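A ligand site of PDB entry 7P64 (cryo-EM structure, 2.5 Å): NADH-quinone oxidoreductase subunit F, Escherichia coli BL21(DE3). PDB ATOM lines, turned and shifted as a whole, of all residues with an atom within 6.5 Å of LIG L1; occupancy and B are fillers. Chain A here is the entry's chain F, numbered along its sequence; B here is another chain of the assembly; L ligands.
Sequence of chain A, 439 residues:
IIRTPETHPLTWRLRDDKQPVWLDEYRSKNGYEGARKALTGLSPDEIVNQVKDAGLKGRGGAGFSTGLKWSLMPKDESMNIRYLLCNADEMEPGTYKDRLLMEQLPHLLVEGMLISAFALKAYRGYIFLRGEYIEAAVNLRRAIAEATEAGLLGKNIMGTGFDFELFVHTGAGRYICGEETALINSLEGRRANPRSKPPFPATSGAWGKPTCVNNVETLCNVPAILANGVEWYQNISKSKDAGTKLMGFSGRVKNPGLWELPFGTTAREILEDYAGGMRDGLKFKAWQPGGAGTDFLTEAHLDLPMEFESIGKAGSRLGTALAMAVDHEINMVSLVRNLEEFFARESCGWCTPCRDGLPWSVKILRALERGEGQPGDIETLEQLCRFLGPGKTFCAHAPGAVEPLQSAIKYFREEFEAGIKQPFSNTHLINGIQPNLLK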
ATOM      1  N   ILE A 176      25.735   2.703  29.726  1.00  0.00           N
ATOM      2  CA  ILE A 176      24.773   3.696  29.256  1.00  0.00           C
ATOM      3  C   ILE A 176      23.789   4.126  30.333  1.00  0.00           C
ATOM      4  O   ILE A 176      23.145   5.173  30.193  1.00  0.00           O
ATOM      5  CB  ILE A 176      24.039   3.143  28.012  1.00  0.00           C
ATOM      6  CG1 ILE A 176      23.455   4.279  27.157  1.00  0.00           C
ATOM      7  CG2 ILE A 176      22.980   2.132  28.404  1.00  0.00           C
ATOM      8  CD1 ILE A 176      24.374   5.443  26.943  1.00  0.00           C
ATOM      9  N   ALA A 192      17.751   0.349  29.344  1.00  0.00           N
ATOM     10  CA  ALA A 192      18.328   1.685  29.542  1.00  0.00           C
ATOM     11  C   ALA A 192      18.626   2.363  28.201  1.00  0.00           C
ATOM     12  O   ALA A 192      19.753   2.673  27.855  1.00  0.00           O
ATOM     13  CB  ALA A 192      19.575   1.594  30.401  1.00  0.00           C
ATOM     14  N   ASN A 193      17.554   2.590  27.450  1.00  0.00           N
ATOM     15  CA  ASN A 193      17.665   3.456  26.287  1.00  0.00           C
ATOM     16  C   ASN A 193      17.480   4.907  26.714  1.00  0.00           C
ATOM     17  O   ASN A 193      16.603   5.199  27.527  1.00  0.00           O
ATOM     18  CB  ASN A 193      16.621   3.095  25.236  1.00  0.00           C
ATOM     19  CG  ASN A 193      16.852   1.740  24.617  1.00  0.00           C
ATOM     20  OD1 ASN A 193      16.146   0.788  24.907  1.00  0.00           O
ATOM     21  ND2 ASN A 193      17.859   1.651  23.754  1.00  0.00           N
ATOM     22  N   PRO A 194      18.286   5.831  26.200  1.00  0.00           N
ATOM     23  CA  PRO A 194      18.067   7.247  26.508  1.00  0.00           C
ATOM     24  C   PRO A 194      16.831   7.784  25.801  1.00  0.00           C
ATOM     25  O   PRO A 194      16.238   7.139  24.946  1.00  0.00           O
ATOM     26  CB  PRO A 194      19.349   7.921  25.996  1.00  0.00           C
ATOM     27  CG  PRO A 194      19.908   6.992  25.007  1.00  0.00           C
ATOM     28  CD  PRO A 194      19.509   5.604  25.419  1.00  0.00           C
ATOM     29  N   GLU A 346      29.402  -1.182  24.810  1.00  0.00           N
ATOM     30  CA  GLU A 346      28.509  -0.517  25.755  1.00  0.00           C
ATOM     31  C   GLU A 346      27.473   0.337  25.049  1.00  0.00           C
ATOM     32  O   GLU A 346      26.809   1.154  25.711  1.00  0.00           O
ATOM     33  CB  GLU A 346      29.315   0.316  26.750  1.00  0.00           C
ATOM     34  CG  GLU A 346      30.181  -0.514  27.674  1.00  0.00           C
ATOM     35  CD  GLU A 346      29.395  -1.535  28.467  1.00  0.00           C
ATOM     36  OE1 GLU A 346      28.320  -1.192  28.989  1.00  0.00           O
ATOM     37  OE2 GLU A 346      29.858  -2.690  28.568  1.00  0.00           O
ATOM     38  N   SER A 347      27.346   0.199  23.739  1.00  0.00           N
ATOM     39  CA  SER A 347      26.252   0.837  23.022  1.00  0.00           C
ATOM     40  C   SER A 347      24.918   0.260  23.482  1.00  0.00           C
ATOM     41  O   SER A 347      24.816  -0.933  23.767  1.00  0.00           O
ATOM     42  CB  SER A 347      26.426   0.634  21.517  1.00  0.00           C
ATOM     43  OG  SER A 347      25.288   1.089  20.809  1.00  0.00           O
ATOM     44  N   CYS A 348      23.905   1.109  23.574  1.00  0.00           N
ATOM     45  CA  CYS A 348      22.593   0.623  23.949  1.00  0.00           C
ATOM     46  C   CYS A 348      21.840   0.018  22.770  1.00  0.00           C
ATOM     47  O   CYS A 348      20.850  -0.694  22.982  1.00  0.00           O
ATOM     48  CB  CYS A 348      21.769   1.742  24.581  1.00  0.00           C
ATOM     49  SG  CYS A 348      20.870   2.755  23.418  1.00  0.00           S
ATOM     50  N   GLY A 349      22.294   0.278  21.545  1.00  0.00           N
ATOM     51  CA  GLY A 349      21.700  -0.318  20.366  1.00  0.00           C
ATOM     52  C   GLY A 349      20.546   0.426  19.767  1.00  0.00           C
ATOM     53  O   GLY A 349      19.907  -0.092  18.839  1.00  0.00           O
ATOM     54  N   TRP A 350      20.238   1.623  20.252  1.00  0.00           N
ATOM     55  CA  TRP A 350      19.064   2.348  19.781  1.00  0.00           C
ATOM     56  C   TRP A 350      19.270   2.901  18.386  1.00  0.00           C
ATOM     57  O   TRP A 350      18.399   2.771  17.518  1.00  0.00           O
ATOM     58  CB  TRP A 350      18.706   3.470  20.746  1.00  0.00           C
ATOM     59  CG  TRP A 350      17.526   4.264  20.362  1.00  0.00           C
ATOM     60  CD1 TRP A 350      17.522   5.564  19.974  1.00  0.00           C
ATOM     61  CD2 TRP A 350      16.165   3.830  20.338  1.00  0.00           C
ATOM     62  NE1 TRP A 350      16.243   5.971  19.704  1.00  0.00           N
ATOM     63  CE2 TRP A 350      15.391   4.921  19.919  1.00  0.00           C
ATOM     64  CE3 TRP A 350      15.538   2.625  20.631  1.00  0.00           C
ATOM     65  CZ2 TRP A 350      14.013   4.839  19.783  1.00  0.00           C
ATOM     66  CZ3 TRP A 350      14.164   2.547  20.487  1.00  0.00           C
ATOM     67  CH2 TRP A 350      13.419   3.647  20.077  1.00  0.00           C
ATOM     68  N   CYS A 351      20.420   3.510  18.126  1.00  0.00           N
ATOM     69  CA  CYS A 351      20.567   4.311  16.920  1.00  0.00           C
ATOM     70  C   CYS A 351      21.718   3.832  16.054  1.00  0.00           C
ATOM     71  O   CYS A 351      22.742   3.339  16.545  1.00  0.00           O
ATOM     72  CB  CYS A 351      20.696   5.813  17.269  1.00  0.00           C
ATOM     73  SG  CYS A 351      22.260   6.413  17.836  1.00  0.00           S
ATOM     74  N   THR A 352      21.526   3.985  14.741  1.00  0.00           N
ATOM     75  CA  THR A 352      22.380   3.349  13.736  1.00  0.00           C
ATOM     76  C   THR A 352      23.850   3.769  13.769  1.00  0.00           C
ATOM     77  O   THR A 352      24.699   2.865  13.683  1.00  0.00           O
ATOM     78  CB  THR A 352      21.771   3.580  12.348  1.00  0.00           C
ATOM     79  OG1 THR A 352      20.436   3.083  12.311  1.00  0.00           O
ATOM     80  CG2 THR A 352      22.595   2.869  11.270  1.00  0.00           C
ATOM     81  N   PRO A 353      24.226   5.059  13.843  1.00  0.00           N
ATOM     82  CA  PRO A 353      25.669   5.385  13.736  1.00  0.00           C
ATOM     83  C   PRO A 353      26.523   4.770  14.827  1.00  0.00           C
ATOM     84  O   PRO A 353      27.524   4.132  14.509  1.00  0.00           O
ATOM     85  CB  PRO A 353      25.680   6.915  13.795  1.00  0.00           C
ATOM     86  CG  PRO A 353      24.371   7.307  13.305  1.00  0.00           C
ATOM     87  CD  PRO A 353      23.457   6.313  13.912  1.00  0.00           C
ATOM     88  N   CYS A 354      26.105   4.864  16.097  1.00  0.00           N
ATOM     89  CA  CYS A 354      26.852   4.221  17.174  1.00  0.00           C
ATOM     90  C   CYS A 354      26.847   2.700  17.013  1.00  0.00           C
ATOM     91  O   CYS A 354      27.915   2.092  16.856  1.00  0.00           O
ATOM     92  CB  CYS A 354      26.248   4.667  18.505  1.00  0.00           C
ATOM     93  SG  CYS A 354      26.668   3.861  20.063  1.00  0.00           S
ATOM     94  N   ARG A 355      25.650   2.111  16.884  1.00  0.00           N
ATOM     95  CA  ARG A 355      25.480   0.665  16.915  1.00  0.00           C
ATOM     96  C   ARG A 355      26.181  -0.036  15.758  1.00  0.00           C
ATOM     97  O   ARG A 355      26.731  -1.126  15.925  1.00  0.00           O
ATOM     98  CB  ARG A 355      23.980   0.326  16.911  1.00  0.00           C
ATOM     99  CG  ARG A 355      23.625  -1.064  16.414  1.00  0.00           C
ATOM    100  CD  ARG A 355      22.139  -1.277  16.286  1.00  0.00           C
ATOM    101  NE  ARG A 355      21.695  -1.029  14.925  1.00  0.00           N
ATOM    102  CZ  ARG A 355      20.883  -0.040  14.565  1.00  0.00           C
ATOM    103  NH1 ARG A 355      20.371   0.784  15.454  1.00  0.00           N
ATOM    104  NH2 ARG A 355      20.588   0.111  13.277  1.00  0.00           N
ATOM    105  N   LEU A 358      30.519   2.096  15.340  1.00  0.00           N
ATOM    106  CA  LEU A 358      31.552   1.750  16.302  1.00  0.00           C
ATOM    107  C   LEU A 358      32.144   0.352  16.096  1.00  0.00           C
ATOM    108  O   LEU A 358      33.379   0.229  16.211  1.00  0.00           O
ATOM    109  CB  LEU A 358      31.018   1.954  17.733  1.00  0.00           C
ATOM    110  CG  LEU A 358      30.826   3.416  18.148  1.00  0.00           C
ATOM    111  CD1 LEU A 358      30.345   3.499  19.585  1.00  0.00           C
ATOM    112  CD2 LEU A 358      32.109   4.205  17.967  1.00  0.00           C
ATOM    113  N   THR A 393      23.841  11.242  16.346  1.00  0.00           N
ATOM    114  CA  THR A 393      23.368  10.099  17.111  1.00  0.00           C
ATOM    115  C   THR A 393      22.291  10.532  18.087  1.00  0.00           C
ATOM    116  O   THR A 393      22.078  11.723  18.330  1.00  0.00           O
ATOM    117  CB  THR A 393      24.525   9.429  17.840  1.00  0.00           C
ATOM    118  OG1 THR A 393      25.133  10.353  18.746  1.00  0.00           O
ATOM    119  CG2 THR A 393      25.560   8.960  16.850  1.00  0.00           C
ATOM    120  N   PHE A 394      21.593   9.545  18.650  1.00  0.00           N
ATOM    121  CA  PHE A 394      20.464   9.847  19.517  1.00  0.00           C
ATOM    122  C   PHE A 394      20.902  10.394  20.869  1.00  0.00           C
ATOM    123  O   PHE A 394      20.168  11.170  21.486  1.00  0.00           O
ATOM    124  CB  PHE A 394      19.610   8.593  19.708  1.00  0.00           C
ATOM    125  CG  PHE A 394      18.285   8.847  20.355  1.00  0.00           C
ATOM    126  CD1 PHE A 394      17.252   9.420  19.647  1.00  0.00           C
ATOM    127  CD2 PHE A 394      18.079   8.513  21.682  1.00  0.00           C
ATOM    128  CE1 PHE A 394      16.035   9.651  20.237  1.00  0.00           C
ATOM    129  CE2 PHE A 394      16.866   8.755  22.280  1.00  0.00           C
ATOM    130  CZ  PHE A 394      15.837   9.311  21.554  1.00  0.00           C
ATOM    131  N   CYS A 395      22.095  10.026  21.338  1.00  0.00           N
ATOM    132  CA  CYS A 395      22.600  10.527  22.611  1.00  0.00           C
ATOM    133  C   CYS A 395      24.081  10.833  22.457  1.00  0.00           C
ATOM    134  O   CYS A 395      24.656  10.713  21.366  1.00  0.00           O
ATOM    135  CB  CYS A 395      22.326   9.527  23.735  1.00  0.00           C
ATOM    136  SG  CYS A 395      23.623   8.335  24.048  1.00  0.00           S
ATOM    137  N   ALA A 396      24.708  11.239  23.553  1.00  0.00           N
ATOM    138  CA  ALA A 396      26.076  11.748  23.539  1.00  0.00           C
ATOM    139  C   ALA A 396      27.114  10.672  23.786  1.00  0.00           C
ATOM    140  O   ALA A 396      28.291  11.000  23.992  1.00  0.00           O
ATOM    141  CB  ALA A 396      26.230  12.861  24.578  1.00  0.00           C
ATOM    142  N   HIS A 397      26.718   9.393  23.791  1.00  0.00           N
ATOM    143  CA  HIS A 397      27.684   8.326  24.013  1.00  0.00           C
ATOM    144  C   HIS A 397      28.643   8.187  22.843  1.00  0.00           C
ATOM    145  O   HIS A 397      29.851   8.017  23.034  1.00  0.00           O
ATOM    146  CB  HIS A 397      26.937   7.016  24.267  1.00  0.00           C
ATOM    147  CG  HIS A 397      27.757   5.788  24.043  1.00  0.00           C
ATOM    148  ND1 HIS A 397      27.795   5.117  22.844  1.00  0.00           N
ATOM    149  CD2 HIS A 397      28.570   5.094  24.881  1.00  0.00           C
ATOM    150  CE1 HIS A 397      28.593   4.073  22.940  1.00  0.00           C
ATOM    151  NE2 HIS A 397      29.074   4.027  24.170  1.00  0.00           N
ATOM    152  N   ALA A 398      28.135   8.264  21.622  1.00  0.00           N
ATOM    153  CA  ALA A 398      28.966   8.100  20.429  1.00  0.00           C
ATOM    154  C   ALA A 398      29.873   9.292  20.097  1.00  0.00           C
ATOM    155  O   ALA A 398      30.987   9.057  19.604  1.00  0.00           O
ATOM    156  CB  ALA A 398      28.075   7.763  19.220  1.00  0.00           C
ATOM    157  N   PRO A 399      29.462  10.563  20.307  1.00  0.00           N
ATOM    158  CA  PRO A 399      30.480  11.633  20.222  1.00  0.00           C
ATOM    159  C   PRO A 399      31.618  11.476  21.212  1.00  0.00           C
ATOM    160  O   PRO A 399      32.777  11.712  20.866  1.00  0.00           O
ATOM    161  CB  PRO A 399      29.655  12.902  20.509  1.00  0.00           C
ATOM    162  CG  PRO A 399      28.330  12.580  20.012  1.00  0.00           C
ATOM    163  CD  PRO A 399      28.105  11.147  20.334  1.00  0.00           C
ATOM    164  N   HIS B 175      24.098  -3.955  22.229  1.00  0.00           N
ATOM    165  CA  HIS B 175      24.674  -3.010  21.283  1.00  0.00           C
ATOM    166  C   HIS B 175      24.409  -3.271  19.806  1.00  0.00           C
ATOM    167  O   HIS B 175      23.644  -2.532  19.186  1.00  0.00           O
ATOM    168  CB  HIS B 175      26.179  -3.049  21.516  1.00  0.00           C
ATOM    169  CG  HIS B 175      26.673  -4.378  21.982  1.00  0.00           C
ATOM    170  ND1 HIS B 175      27.000  -5.399  21.113  1.00  0.00           N
ATOM    171  CD2 HIS B 175      26.854  -4.883  23.230  1.00  0.00           C
ATOM    172  CE1 HIS B 175      27.372  -6.468  21.798  1.00  0.00           C
ATOM    173  NE2 HIS B 175      27.297  -6.177  23.090  1.00  0.00           N
HETATM  174 FE1  LIG L   1      22.697   5.772  20.025  1.00  0.00          FE
HETATM  175 FE2  LIG L   1      24.758   4.616  21.129  1.00  0.00          FE
HETATM  176 FE3  LIG L   1      23.447   6.553  22.562  1.00  0.00          FE
HETATM  177 FE4  LIG L   1      22.304   4.195  22.266  1.00  0.00          FE
HETATM  178  S1  LIG L   1      24.279   4.572  23.386  1.00  0.00           S
HETATM  179  S2  LIG L   1      21.303   6.208  21.799  1.00  0.00           S
HETATM  180  S3  LIG L   1      22.977   3.500  20.174  1.00  0.00           S
HETATM  181  S4  LIG L   1      24.634   6.850  20.624  1.00  0.00           S
HETATM  182  N1  LG2 L   2      26.899  11.286  34.964  1.00  0.00           N
HETATM  183  C1  LG2 L   2      27.230  10.726  36.179  1.00  0.00           C
HETATM  184  O1  LG2 L   2      27.133  11.408  37.189  1.00  0.00           O
HETATM  185  N2  LG2 L   2      27.653   9.430  36.248  1.00  0.00           N
HETATM  186  C2  LG2 L   2      27.745   8.674  35.094  1.00  0.00           C
HETATM  187  O2  LG2 L   2      28.124   7.514  35.157  1.00  0.00           O
HETATM  188  C3  LG2 L   2      27.419   9.237  33.871  1.00  0.00           C
HETATM  189  N3  LG2 L   2      27.503   8.499  32.721  1.00  0.00           N
HETATM  190  C4  LG2 L   2      27.173   9.059  31.506  1.00  0.00           C
HETATM  191  C5  LG2 L   2      27.275   8.283  30.363  1.00  0.00           C
HETATM  192  C6  LG2 L   2      26.949   8.838  29.125  1.00  0.00           C
HETATM  193  C7  LG2 L   2      27.068   7.986  27.898  1.00  0.00           C
HETATM  194  C8  LG2 L   2      26.524  10.156  29.051  1.00  0.00           C
HETATM  195  C9  LG2 L   2      26.169  10.759  27.729  1.00  0.00           C
HETATM  196  C10 LG2 L   2      26.420  10.919  30.201  1.00  0.00           C
HETATM  197  C11 LG2 L   2      26.742  10.373  31.440  1.00  0.00           C
HETATM  198  N4  LG2 L   2      26.646  11.126  32.602  1.00  0.00           N
HETATM  199  C12 LG2 L   2      26.988  10.551  33.805  1.00  0.00           C
HETATM  200  C13 LG2 L   2      26.188  12.563  32.583  1.00  0.00           C
HETATM  201  C14 LG2 L   2      24.676  12.622  32.821  1.00  0.00           C
HETATM  202  O3  LG2 L   2      24.022  12.646  31.578  1.00  0.00           O
HETATM  203  C15 LG2 L   2      24.258  13.846  33.634  1.00  0.00           C
HETATM  204  O4  LG2 L   2      24.886  15.004  33.125  1.00  0.00           O
HETATM  205  C16 LG2 L   2      24.608  13.672  35.104  1.00  0.00           C
HETATM  206  O5  LG2 L   2      24.207  12.402  35.527  1.00  0.00           O
HETATM  207  C17 LG2 L   2      23.966  14.716  36.007  1.00  0.00           C
HETATM  208  O6  LG2 L   2      24.355  16.001  35.595  1.00  0.00           O
HETATM  209  P1  LG2 L   2      25.116  16.987  36.615  1.00  0.00           P
HETATM  210  O7  LG2 L   2      26.578  16.920  36.309  1.00  0.00           O
HETATM  211  O8  LG2 L   2      24.599  18.396  36.440  1.00  0.00           O
HETATM  212  O9  LG2 L   2      24.898  16.544  38.038  1.00  0.00           O
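Merely in contact with LIG L1: Ile 176 (3.7 Å), Pro 194 (3.6 Å), Thr 393 (3.8 Å), Phe 394 (3.6 Å) and Ala 398 (3.8 Å).
Hydrophobic or aromatic side chains within 4 Å of LIG L1: Ile 176, Pro 194, Trp 350, Phe 394, His 397 and Ala 398.
13 residues have an atom within 4 Å of LIG L1: Ile 176, Pro 194, Ser 347, Cys 348, Gly 349, Trp 350, Cys 351, Cys 354, Thr 393, Phe 394, Cys 395, His 397 and Ala 398.
The nearest printed residue that does not touch LIG L1 is Arg 355 (4.5 Å).
The backbone NH (N) of Cys 348 lies close to a sulfur (S1) of LIG L1 (3.5 Å).
The side-chain sulfur of Cys 395 binds an iron atom (FE3) of LIG L1 (2.3 Å).
FE4 of LIG L1 is bound by SG of Cys 348, 2.3 Å away.
The side-chain sulfur of Cys 354 binds an iron atom (FE2) of LIG L1, at 2.3 Å.
A sulfur (S3) of LIG L1 sits close to the side-chain hydroxyl of Ser 347.
N of Gly 349 sits close to S3 of LIG L1, at 3.6 Å.
S3 of LIG L1 lies close to N of Trp 350 (3.3 Å).
A ring nitrogen (ND1) of His 397 lies close to a sulfur (S1) of LIG L1 (3.6 Å).
The backbone NH of Cys 351 lies close to a sulfur (S3) of LIG L1 (3.3 Å).
FE1 of LIG L1 is bound by SG of Cys 351.
The backbone carbonyl oxygen (O) of Ser 347 sits close to the backbone NH (N) of His 175 of chain B, 3.5 Å away.
O of Cys 395 lies within hydrogen-bond range of OG1 of Thr 393, at 2.7 Å.
The side-chain sulfur (SG) of Cys 354 lies close to the side-chain hydroxyl (OG) of Ser 347 (3.2 Å).
The side-chain hydroxyl (OG) of Ser 347 lies within hydrogen-bond range of the backbone NH (N) of Gly 349 (3.2 Å).
The side-chain sulfur of Cys 354 sits close to a ring nitrogen (ND1) of His 397, 3.3 Å away.
N of His 397 lies close to SG of Cys 395.
The backbone carbonyl oxygen of Trp 350 lies within hydrogen-bond range of the guanidinium group of Arg 355 (3.5 Å).
The side-chain sulfur (SG) of Cys 348 lies close to the backbone NH (N) of Trp 350, 3.4 Å away.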
